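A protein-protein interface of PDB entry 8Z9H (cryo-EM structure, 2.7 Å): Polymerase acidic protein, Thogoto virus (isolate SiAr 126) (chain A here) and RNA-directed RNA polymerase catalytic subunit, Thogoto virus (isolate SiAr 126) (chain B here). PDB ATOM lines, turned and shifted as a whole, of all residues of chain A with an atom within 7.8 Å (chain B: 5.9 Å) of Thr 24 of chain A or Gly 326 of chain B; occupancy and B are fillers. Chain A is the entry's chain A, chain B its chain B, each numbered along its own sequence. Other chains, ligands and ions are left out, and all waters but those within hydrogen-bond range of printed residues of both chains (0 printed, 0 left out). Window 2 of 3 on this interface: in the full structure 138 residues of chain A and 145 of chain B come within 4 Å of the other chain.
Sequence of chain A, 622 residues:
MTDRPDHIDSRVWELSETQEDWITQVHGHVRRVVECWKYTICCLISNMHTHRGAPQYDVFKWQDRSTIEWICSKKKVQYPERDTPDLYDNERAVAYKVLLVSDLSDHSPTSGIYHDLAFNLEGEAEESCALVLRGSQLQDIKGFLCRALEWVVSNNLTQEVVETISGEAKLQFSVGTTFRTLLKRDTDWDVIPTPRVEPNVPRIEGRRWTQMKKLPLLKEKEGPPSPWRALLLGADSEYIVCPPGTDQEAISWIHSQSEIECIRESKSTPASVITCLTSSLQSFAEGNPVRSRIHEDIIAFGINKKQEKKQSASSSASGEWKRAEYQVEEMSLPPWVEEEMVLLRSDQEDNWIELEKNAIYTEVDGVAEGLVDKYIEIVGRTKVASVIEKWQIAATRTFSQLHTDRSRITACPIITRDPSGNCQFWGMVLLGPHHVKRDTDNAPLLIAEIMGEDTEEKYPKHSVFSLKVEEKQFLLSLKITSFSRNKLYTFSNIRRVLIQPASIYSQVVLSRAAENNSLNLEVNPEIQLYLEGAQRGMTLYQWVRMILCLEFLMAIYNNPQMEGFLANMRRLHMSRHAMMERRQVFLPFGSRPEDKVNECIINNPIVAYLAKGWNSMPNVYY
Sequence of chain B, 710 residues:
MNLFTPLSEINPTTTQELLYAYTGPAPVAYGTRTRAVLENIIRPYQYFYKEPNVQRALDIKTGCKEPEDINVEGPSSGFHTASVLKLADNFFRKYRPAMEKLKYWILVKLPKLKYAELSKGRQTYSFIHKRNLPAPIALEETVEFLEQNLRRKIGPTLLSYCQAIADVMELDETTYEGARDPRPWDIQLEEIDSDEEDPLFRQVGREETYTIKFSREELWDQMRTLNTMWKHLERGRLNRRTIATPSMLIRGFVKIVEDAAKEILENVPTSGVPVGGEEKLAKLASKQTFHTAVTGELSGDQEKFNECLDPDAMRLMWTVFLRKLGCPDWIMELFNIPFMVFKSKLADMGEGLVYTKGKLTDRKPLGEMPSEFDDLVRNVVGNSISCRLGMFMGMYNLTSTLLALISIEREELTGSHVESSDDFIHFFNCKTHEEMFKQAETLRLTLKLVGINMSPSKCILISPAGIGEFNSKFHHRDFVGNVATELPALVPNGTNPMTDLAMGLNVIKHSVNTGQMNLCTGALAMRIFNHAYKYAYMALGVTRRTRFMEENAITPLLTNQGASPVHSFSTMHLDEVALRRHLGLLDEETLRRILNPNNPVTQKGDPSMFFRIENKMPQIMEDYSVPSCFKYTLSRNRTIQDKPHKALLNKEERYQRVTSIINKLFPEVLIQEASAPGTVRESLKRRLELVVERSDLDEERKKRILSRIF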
ATOM      1  N   GLU A  20      13.929  30.662  33.084  1.00  0.00           N
ATOM      2  CA  GLU A  20      14.096  30.161  31.730  1.00  0.00           C
ATOM      3  C   GLU A  20      14.811  28.821  31.786  1.00  0.00           C
ATOM      4  O   GLU A  20      15.541  28.529  32.736  1.00  0.00           O
ATOM      5  CB  GLU A  20      14.886  31.140  30.849  1.00  0.00           C
ATOM      6  CG  GLU A  20      14.224  32.495  30.669  1.00  0.00           C
ATOM      7  CD  GLU A  20      15.004  33.404  29.742  1.00  0.00           C
ATOM      8  OE1 GLU A  20      15.823  32.890  28.952  1.00  0.00           O
ATOM      9  OE2 GLU A  20      14.798  34.635  29.801  1.00  0.00           O
ATOM     10  N   ASP A  21      14.588  28.006  30.759  1.00  0.00           N
ATOM     11  CA  ASP A  21      15.234  26.699  30.660  1.00  0.00           C
ATOM     12  C   ASP A  21      16.620  26.915  30.066  1.00  0.00           C
ATOM     13  O   ASP A  21      16.814  26.900  28.850  1.00  0.00           O
ATOM     14  CB  ASP A  21      14.391  25.747  29.822  1.00  0.00           C
ATOM     15  CG  ASP A  21      14.881  24.319  29.895  1.00  0.00           C
ATOM     16  OD1 ASP A  21      14.694  23.678  30.949  1.00  0.00           O
ATOM     17  OD2 ASP A  21      15.445  23.834  28.895  1.00  0.00           O
ATOM     18  N   TRP A  22      17.601  27.121  30.947  1.00  0.00           N
ATOM     19  CA  TRP A  22      18.935  27.519  30.514  1.00  0.00           C
ATOM     20  C   TRP A  22      19.702  26.394  29.836  1.00  0.00           C
ATOM     21  O   TRP A  22      20.678  26.666  29.132  1.00  0.00           O
ATOM     22  CB  TRP A  22      19.743  28.035  31.705  1.00  0.00           C
ATOM     23  CG  TRP A  22      19.009  29.017  32.564  1.00  0.00           C
ATOM     24  CD1 TRP A  22      18.572  28.819  33.840  1.00  0.00           C
ATOM     25  CD2 TRP A  22      18.636  30.354  32.214  1.00  0.00           C
ATOM     26  NE1 TRP A  22      17.944  29.948  34.305  1.00  0.00           N
ATOM     27  CE2 TRP A  22      17.970  30.905  33.326  1.00  0.00           C
ATOM     28  CE3 TRP A  22      18.797  31.138  31.069  1.00  0.00           C
ATOM     29  CZ2 TRP A  22      17.468  32.202  33.327  1.00  0.00           C
ATOM     30  CZ3 TRP A  22      18.296  32.425  31.072  1.00  0.00           C
ATOM     31  CH2 TRP A  22      17.639  32.944  32.193  1.00  0.00           C
ATOM     32  N   ILE A  23      19.293  25.139  30.033  1.00  0.00           N
ATOM     33  CA  ILE A  23      20.070  24.020  29.511  1.00  0.00           C
ATOM     34  C   ILE A  23      20.021  23.988  27.986  1.00  0.00           C
ATOM     35  O   ILE A  23      21.013  23.650  27.329  1.00  0.00           O
ATOM     36  CB  ILE A  23      19.594  22.696  30.140  1.00  0.00           C
ATOM     37  CG1 ILE A  23      20.540  21.553  29.771  1.00  0.00           C
ATOM     38  CG2 ILE A  23      18.162  22.373  29.742  1.00  0.00           C
ATOM     39  CD1 ILE A  23      21.935  21.718  30.322  1.00  0.00           C
ATOM     40  N   THR A  24      18.879  24.343  27.396  1.00  0.00           N
ATOM     41  CA  THR A  24      18.733  24.302  25.946  1.00  0.00           C
ATOM     42  C   THR A  24      19.240  25.559  25.249  1.00  0.00           C
ATOM     43  O   THR A  24      19.417  25.535  24.026  1.00  0.00           O
ATOM     44  CB  THR A  24      17.268  24.078  25.563  1.00  0.00           C
ATOM     45  OG1 THR A  24      16.482  25.199  25.984  1.00  0.00           O
ATOM     46  CG2 THR A  24      16.735  22.812  26.206  1.00  0.00           C
ATOM     47  N   GLN A  25      19.473  26.642  25.979  1.00  0.00           N
ATOM     48  CA  GLN A  25      19.922  27.879  25.360  1.00  0.00           C
ATOM     49  C   GLN A  25      21.432  27.870  25.164  1.00  0.00           C
ATOM     50  O   GLN A  25      22.172  27.196  25.884  1.00  0.00           O
ATOM     51  CB  GLN A  25      19.513  29.084  26.205  1.00  0.00           C
ATOM     52  CG  GLN A  25      18.029  29.146  26.511  1.00  0.00           C
ATOM     53  CD  GLN A  25      17.665  30.334  27.373  1.00  0.00           C
ATOM     54  OE1 GLN A  25      18.530  31.113  27.771  1.00  0.00           O
ATOM     55  NE2 GLN A  25      16.380  30.481  27.667  1.00  0.00           N
ATOM     56  N   VAL A  26      21.885  28.630  24.167  1.00  0.00           N
ATOM     57  CA  VAL A  26      23.313  28.758  23.911  1.00  0.00           C
ATOM     58  C   VAL A  26      23.957  29.544  25.043  1.00  0.00           C
ATOM     59  O   VAL A  26      23.509  30.646  25.386  1.00  0.00           O
ATOM     60  CB  VAL A  26      23.560  29.435  22.555  1.00  0.00           C
ATOM     61  CG1 VAL A  26      25.044  29.647  22.337  1.00  0.00           C
ATOM     62  CG2 VAL A  26      22.964  28.603  21.434  1.00  0.00           C
ATOM     63  N   HIS A  27      25.018  28.983  25.621  1.00  0.00           N
ATOM     64  CA  HIS A  27      25.699  29.567  26.774  1.00  0.00           C
ATOM     65  C   HIS A  27      24.701  29.839  27.899  1.00  0.00           C
ATOM     66  O   HIS A  27      24.459  30.980  28.296  1.00  0.00           O
ATOM     67  CB  HIS A  27      26.453  30.839  26.379  1.00  0.00           C
ATOM     68  CG  HIS A  27      27.589  30.598  25.435  1.00  0.00           C
ATOM     69  ND1 HIS A  27      27.599  31.083  24.145  1.00  0.00           N
ATOM     70  CD2 HIS A  27      28.752  29.924  25.593  1.00  0.00           C
ATOM     71  CE1 HIS A  27      28.720  30.718  23.549  1.00  0.00           C
ATOM     72  NE2 HIS A  27      29.438  30.014  24.406  1.00  0.00           N
ATOM     73  N   GLY A  28      24.111  28.752  28.398  1.00  0.00           N
ATOM     74  CA  GLY A  28      23.045  28.881  29.378  1.00  0.00           C
ATOM     75  C   GLY A  28      23.480  29.601  30.639  1.00  0.00           C
ATOM     76  O   GLY A  28      22.742  30.430  31.176  1.00  0.00           O
ATOM     77  N   LEU A 171      25.859  27.167  18.125  1.00  0.00           N
ATOM     78  CA  LEU A 171      25.474  26.028  18.955  1.00  0.00           C
ATOM     79  C   LEU A 171      26.636  25.398  19.715  1.00  0.00           C
ATOM     80  O   LEU A 171      26.410  24.399  20.408  1.00  0.00           O
ATOM     81  CB  LEU A 171      24.792  24.965  18.093  1.00  0.00           C
ATOM     82  CG  LEU A 171      23.323  25.209  17.747  1.00  0.00           C
ATOM     83  CD1 LEU A 171      22.668  23.923  17.269  1.00  0.00           C
ATOM     84  CD2 LEU A 171      22.575  25.779  18.940  1.00  0.00           C
ATOM     85  N   LYS B 103      23.661  18.128  35.347  1.00  0.00           N
ATOM     86  CA  LYS B 103      23.171  19.335  34.686  1.00  0.00           C
ATOM     87  C   LYS B 103      24.040  20.537  35.028  1.00  0.00           C
ATOM     88  O   LYS B 103      24.360  21.352  34.153  1.00  0.00           O
ATOM     89  CB  LYS B 103      21.718  19.597  35.080  1.00  0.00           C
ATOM     90  CG  LYS B 103      21.188  20.942  34.610  1.00  0.00           C
ATOM     91  CD  LYS B 103      19.683  21.044  34.785  1.00  0.00           C
ATOM     92  CE  LYS B 103      18.958  20.022  33.930  1.00  0.00           C
ATOM     93  NZ  LYS B 103      17.513  20.347  33.787  1.00  0.00           N
ATOM     94  N   PHE B 321      20.197   9.461  29.517  1.00  0.00           N
ATOM     95  CA  PHE B 321      20.516  10.383  30.604  1.00  0.00           C
ATOM     96  C   PHE B 321      20.367  11.832  30.160  1.00  0.00           C
ATOM     97  O   PHE B 321      19.784  12.655  30.875  1.00  0.00           O
ATOM     98  CB  PHE B 321      21.937  10.137  31.113  1.00  0.00           C
ATOM     99  CG  PHE B 321      22.082   8.900  31.945  1.00  0.00           C
ATOM    100  CD1 PHE B 321      20.972   8.262  32.467  1.00  0.00           C
ATOM    101  CD2 PHE B 321      23.335   8.385  32.220  1.00  0.00           C
ATOM    102  CE1 PHE B 321      21.110   7.127  33.234  1.00  0.00           C
ATOM    103  CE2 PHE B 321      23.479   7.254  32.989  1.00  0.00           C
ATOM    104  CZ  PHE B 321      22.365   6.623  33.494  1.00  0.00           C
ATOM    105  N   LEU B 322      20.891  12.164  28.981  1.00  0.00           N
ATOM    106  CA  LEU B 322      20.834  13.539  28.507  1.00  0.00           C
ATOM    107  C   LEU B 322      19.470  13.910  27.942  1.00  0.00           C
ATOM    108  O   LEU B 322      19.171  15.101  27.815  1.00  0.00           O
ATOM    109  CB  LEU B 322      21.911  13.780  27.449  1.00  0.00           C
ATOM    110  CG  LEU B 322      23.346  13.495  27.896  1.00  0.00           C
ATOM    111  CD1 LEU B 322      24.226  13.156  26.703  1.00  0.00           C
ATOM    112  CD2 LEU B 322      23.919  14.655  28.684  1.00  0.00           C
ATOM    113  N   ARG B 323      18.637  12.924  27.611  1.00  0.00           N
ATOM    114  CA  ARG B 323      17.315  13.216  27.076  1.00  0.00           C
ATOM    115  C   ARG B 323      16.306  13.442  28.190  1.00  0.00           C
ATOM    116  O   ARG B 323      15.420  14.295  28.064  1.00  0.00           O
ATOM    117  CB  ARG B 323      16.874  12.078  26.157  1.00  0.00           C
ATOM    118  CG  ARG B 323      15.405  12.068  25.791  1.00  0.00           C
ATOM    119  CD  ARG B 323      15.120  10.902  24.865  1.00  0.00           C
ATOM    120  NE  ARG B 323      15.810  11.059  23.590  1.00  0.00           N
ATOM    121  CZ  ARG B 323      16.106  10.060  22.770  1.00  0.00           C
ATOM    122  NH1 ARG B 323      15.796   8.809  23.064  1.00  0.00           N
ATOM    123  NH2 ARG B 323      16.734  10.324  21.627  1.00  0.00           N
ATOM    124  N   LYS B 324      16.423  12.698  29.292  1.00  0.00           N
ATOM    125  CA  LYS B 324      15.545  12.962  30.423  1.00  0.00           C
ATOM    126  C   LYS B 324      15.934  14.230  31.171  1.00  0.00           C
ATOM    127  O   LYS B 324      15.132  14.740  31.961  1.00  0.00           O
ATOM    128  CB  LYS B 324      15.529  11.774  31.379  1.00  0.00           C
ATOM    129  CG  LYS B 324      14.852  10.546  30.809  1.00  0.00           C
ATOM    130  CD  LYS B 324      14.711   9.476  31.865  1.00  0.00           C
ATOM    131  CE  LYS B 324      13.638   9.866  32.868  1.00  0.00           C
ATOM    132  NZ  LYS B 324      12.284   9.878  32.250  1.00  0.00           N
ATOM    133  N   LEU B 325      17.140  14.746  30.945  1.00  0.00           N
ATOM    134  CA  LEU B 325      17.565  16.007  31.536  1.00  0.00           C
ATOM    135  C   LEU B 325      17.172  17.217  30.702  1.00  0.00           C
ATOM    136  O   LEU B 325      17.367  18.350  31.152  1.00  0.00           O
ATOM    137  CB  LEU B 325      19.083  16.012  31.740  1.00  0.00           C
ATOM    138  CG  LEU B 325      19.595  15.629  33.129  1.00  0.00           C
ATOM    139  CD1 LEU B 325      21.078  15.929  33.246  1.00  0.00           C
ATOM    140  CD2 LEU B 325      18.811  16.352  34.210  1.00  0.00           C
ATOM    141  N   GLY B 326      16.627  17.008  29.506  1.00  0.00           N
ATOM    142  CA  GLY B 326      16.254  18.116  28.651  1.00  0.00           C
ATOM    143  C   GLY B 326      17.390  18.732  27.872  1.00  0.00           C
ATOM    144  O   GLY B 326      17.236  19.840  27.351  1.00  0.00           O
ATOM    145  N   CYS B 327      18.531  18.054  27.778  1.00  0.00           N
ATOM    146  CA  CYS B 327      19.666  18.605  27.057  1.00  0.00           C
ATOM    147  C   CYS B 327      19.361  18.700  25.562  1.00  0.00           C
ATOM    148  O   CYS B 327      18.609  17.886  25.020  1.00  0.00           O
ATOM    149  CB  CYS B 327      20.908  17.747  27.279  1.00  0.00           C
ATOM    150  SG  CYS B 327      21.367  17.535  29.013  1.00  0.00           S
ATOM    151  N   PRO B 328      19.931  19.692  24.876  1.00  0.00           N
ATOM    152  CA  PRO B 328      19.684  19.833  23.434  1.00  0.00           C
ATOM    153  C   PRO B 328      20.417  18.794  22.601  1.00  0.00           C
ATOM    154  O   PRO B 328      21.066  17.894  23.142  1.00  0.00           O
ATOM    155  CB  PRO B 328      20.182  21.251  23.136  1.00  0.00           C
ATOM    156  CG  PRO B 328      21.214  21.500  24.174  1.00  0.00           C
ATOM    157  CD  PRO B 328      20.728  20.807  25.411  1.00  0.00           C
ATOM    158  N   TRP B 330      22.995  19.089  20.445  1.00  0.00           N
ATOM    159  CA  TRP B 330      24.446  19.167  20.304  1.00  0.00           C
ATOM    160  C   TRP B 330      25.163  18.470  21.454  1.00  0.00           C
ATOM    161  O   TRP B 330      26.217  17.858  21.241  1.00  0.00           O
ATOM    162  CB  TRP B 330      24.890  20.624  20.176  1.00  0.00           C
ATOM    163  CG  TRP B 330      24.804  21.431  21.433  1.00  0.00           C
ATOM    164  CD1 TRP B 330      23.712  22.091  21.910  1.00  0.00           C
ATOM    165  CD2 TRP B 330      25.865  21.691  22.362  1.00  0.00           C
ATOM    166  NE1 TRP B 330      24.020  22.733  23.083  1.00  0.00           N
ATOM    167  CE2 TRP B 330      25.336  22.503  23.383  1.00  0.00           C
ATOM    168  CE3 TRP B 330      27.207  21.308  22.433  1.00  0.00           C
ATOM    169  CZ2 TRP B 330      26.102  22.940  24.460  1.00  0.00           C
ATOM    170  CZ3 TRP B 330      27.965  21.743  23.503  1.00  0.00           C
ATOM    171  CH2 TRP B 330      27.411  22.552  24.501  1.00  0.00           C
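Of chain B, only Gly 326 comes within 4 Å of Thr 24 of chain A.
Val 26 of chain A touches none of the printed residues of chain B.
Printed residues of chain B within 4 Å of Leu 171 of chain A: Trp 330 (3.4 Å).
Of the printed residues of chain A, Trp 330 of chain B touches Leu 171.
The nearest residue of chain B that does not touch Thr 24 of chain A is Pro 328 of chain B (4.1 Å).
Of the 10 printed residues of chain A, 3 touch a printed residue of chain B.
Hydrophobic or aromatic side chains of chain A within 4 Å of the printed part of chain B: Ile 23.
Printed residues of chain B that touch a printed residue of chain A: Gly 326, Pro 328 and Trp 330.
Hydrophobic or aromatic side chains of chain B that line the printed part of chain A: Pro 328 and Trp 330.
Along chain B the printed residues that touch a printed residue of chain A span positions 326 to 330.
The backbone carbonyl oxygen (O) of Asp 21 of chain A sits at hydrogen-bond distance from the side-chain hydroxyl (OG1) of Thr 24 of chain A, 3.3 Å away.
Gly 326 of chain B touches Ile 23 of chain A.
Pro 328 of chain B touches Ile 23 of chain A (CD to O, 3.4 Å).
Gly 326 of chain B touches Thr 24 of chain A (O to CG2, 3.2 Å).
CD2 of Trp 330 of chain B touches O of Leu 171 of chain A (3.4 Å).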
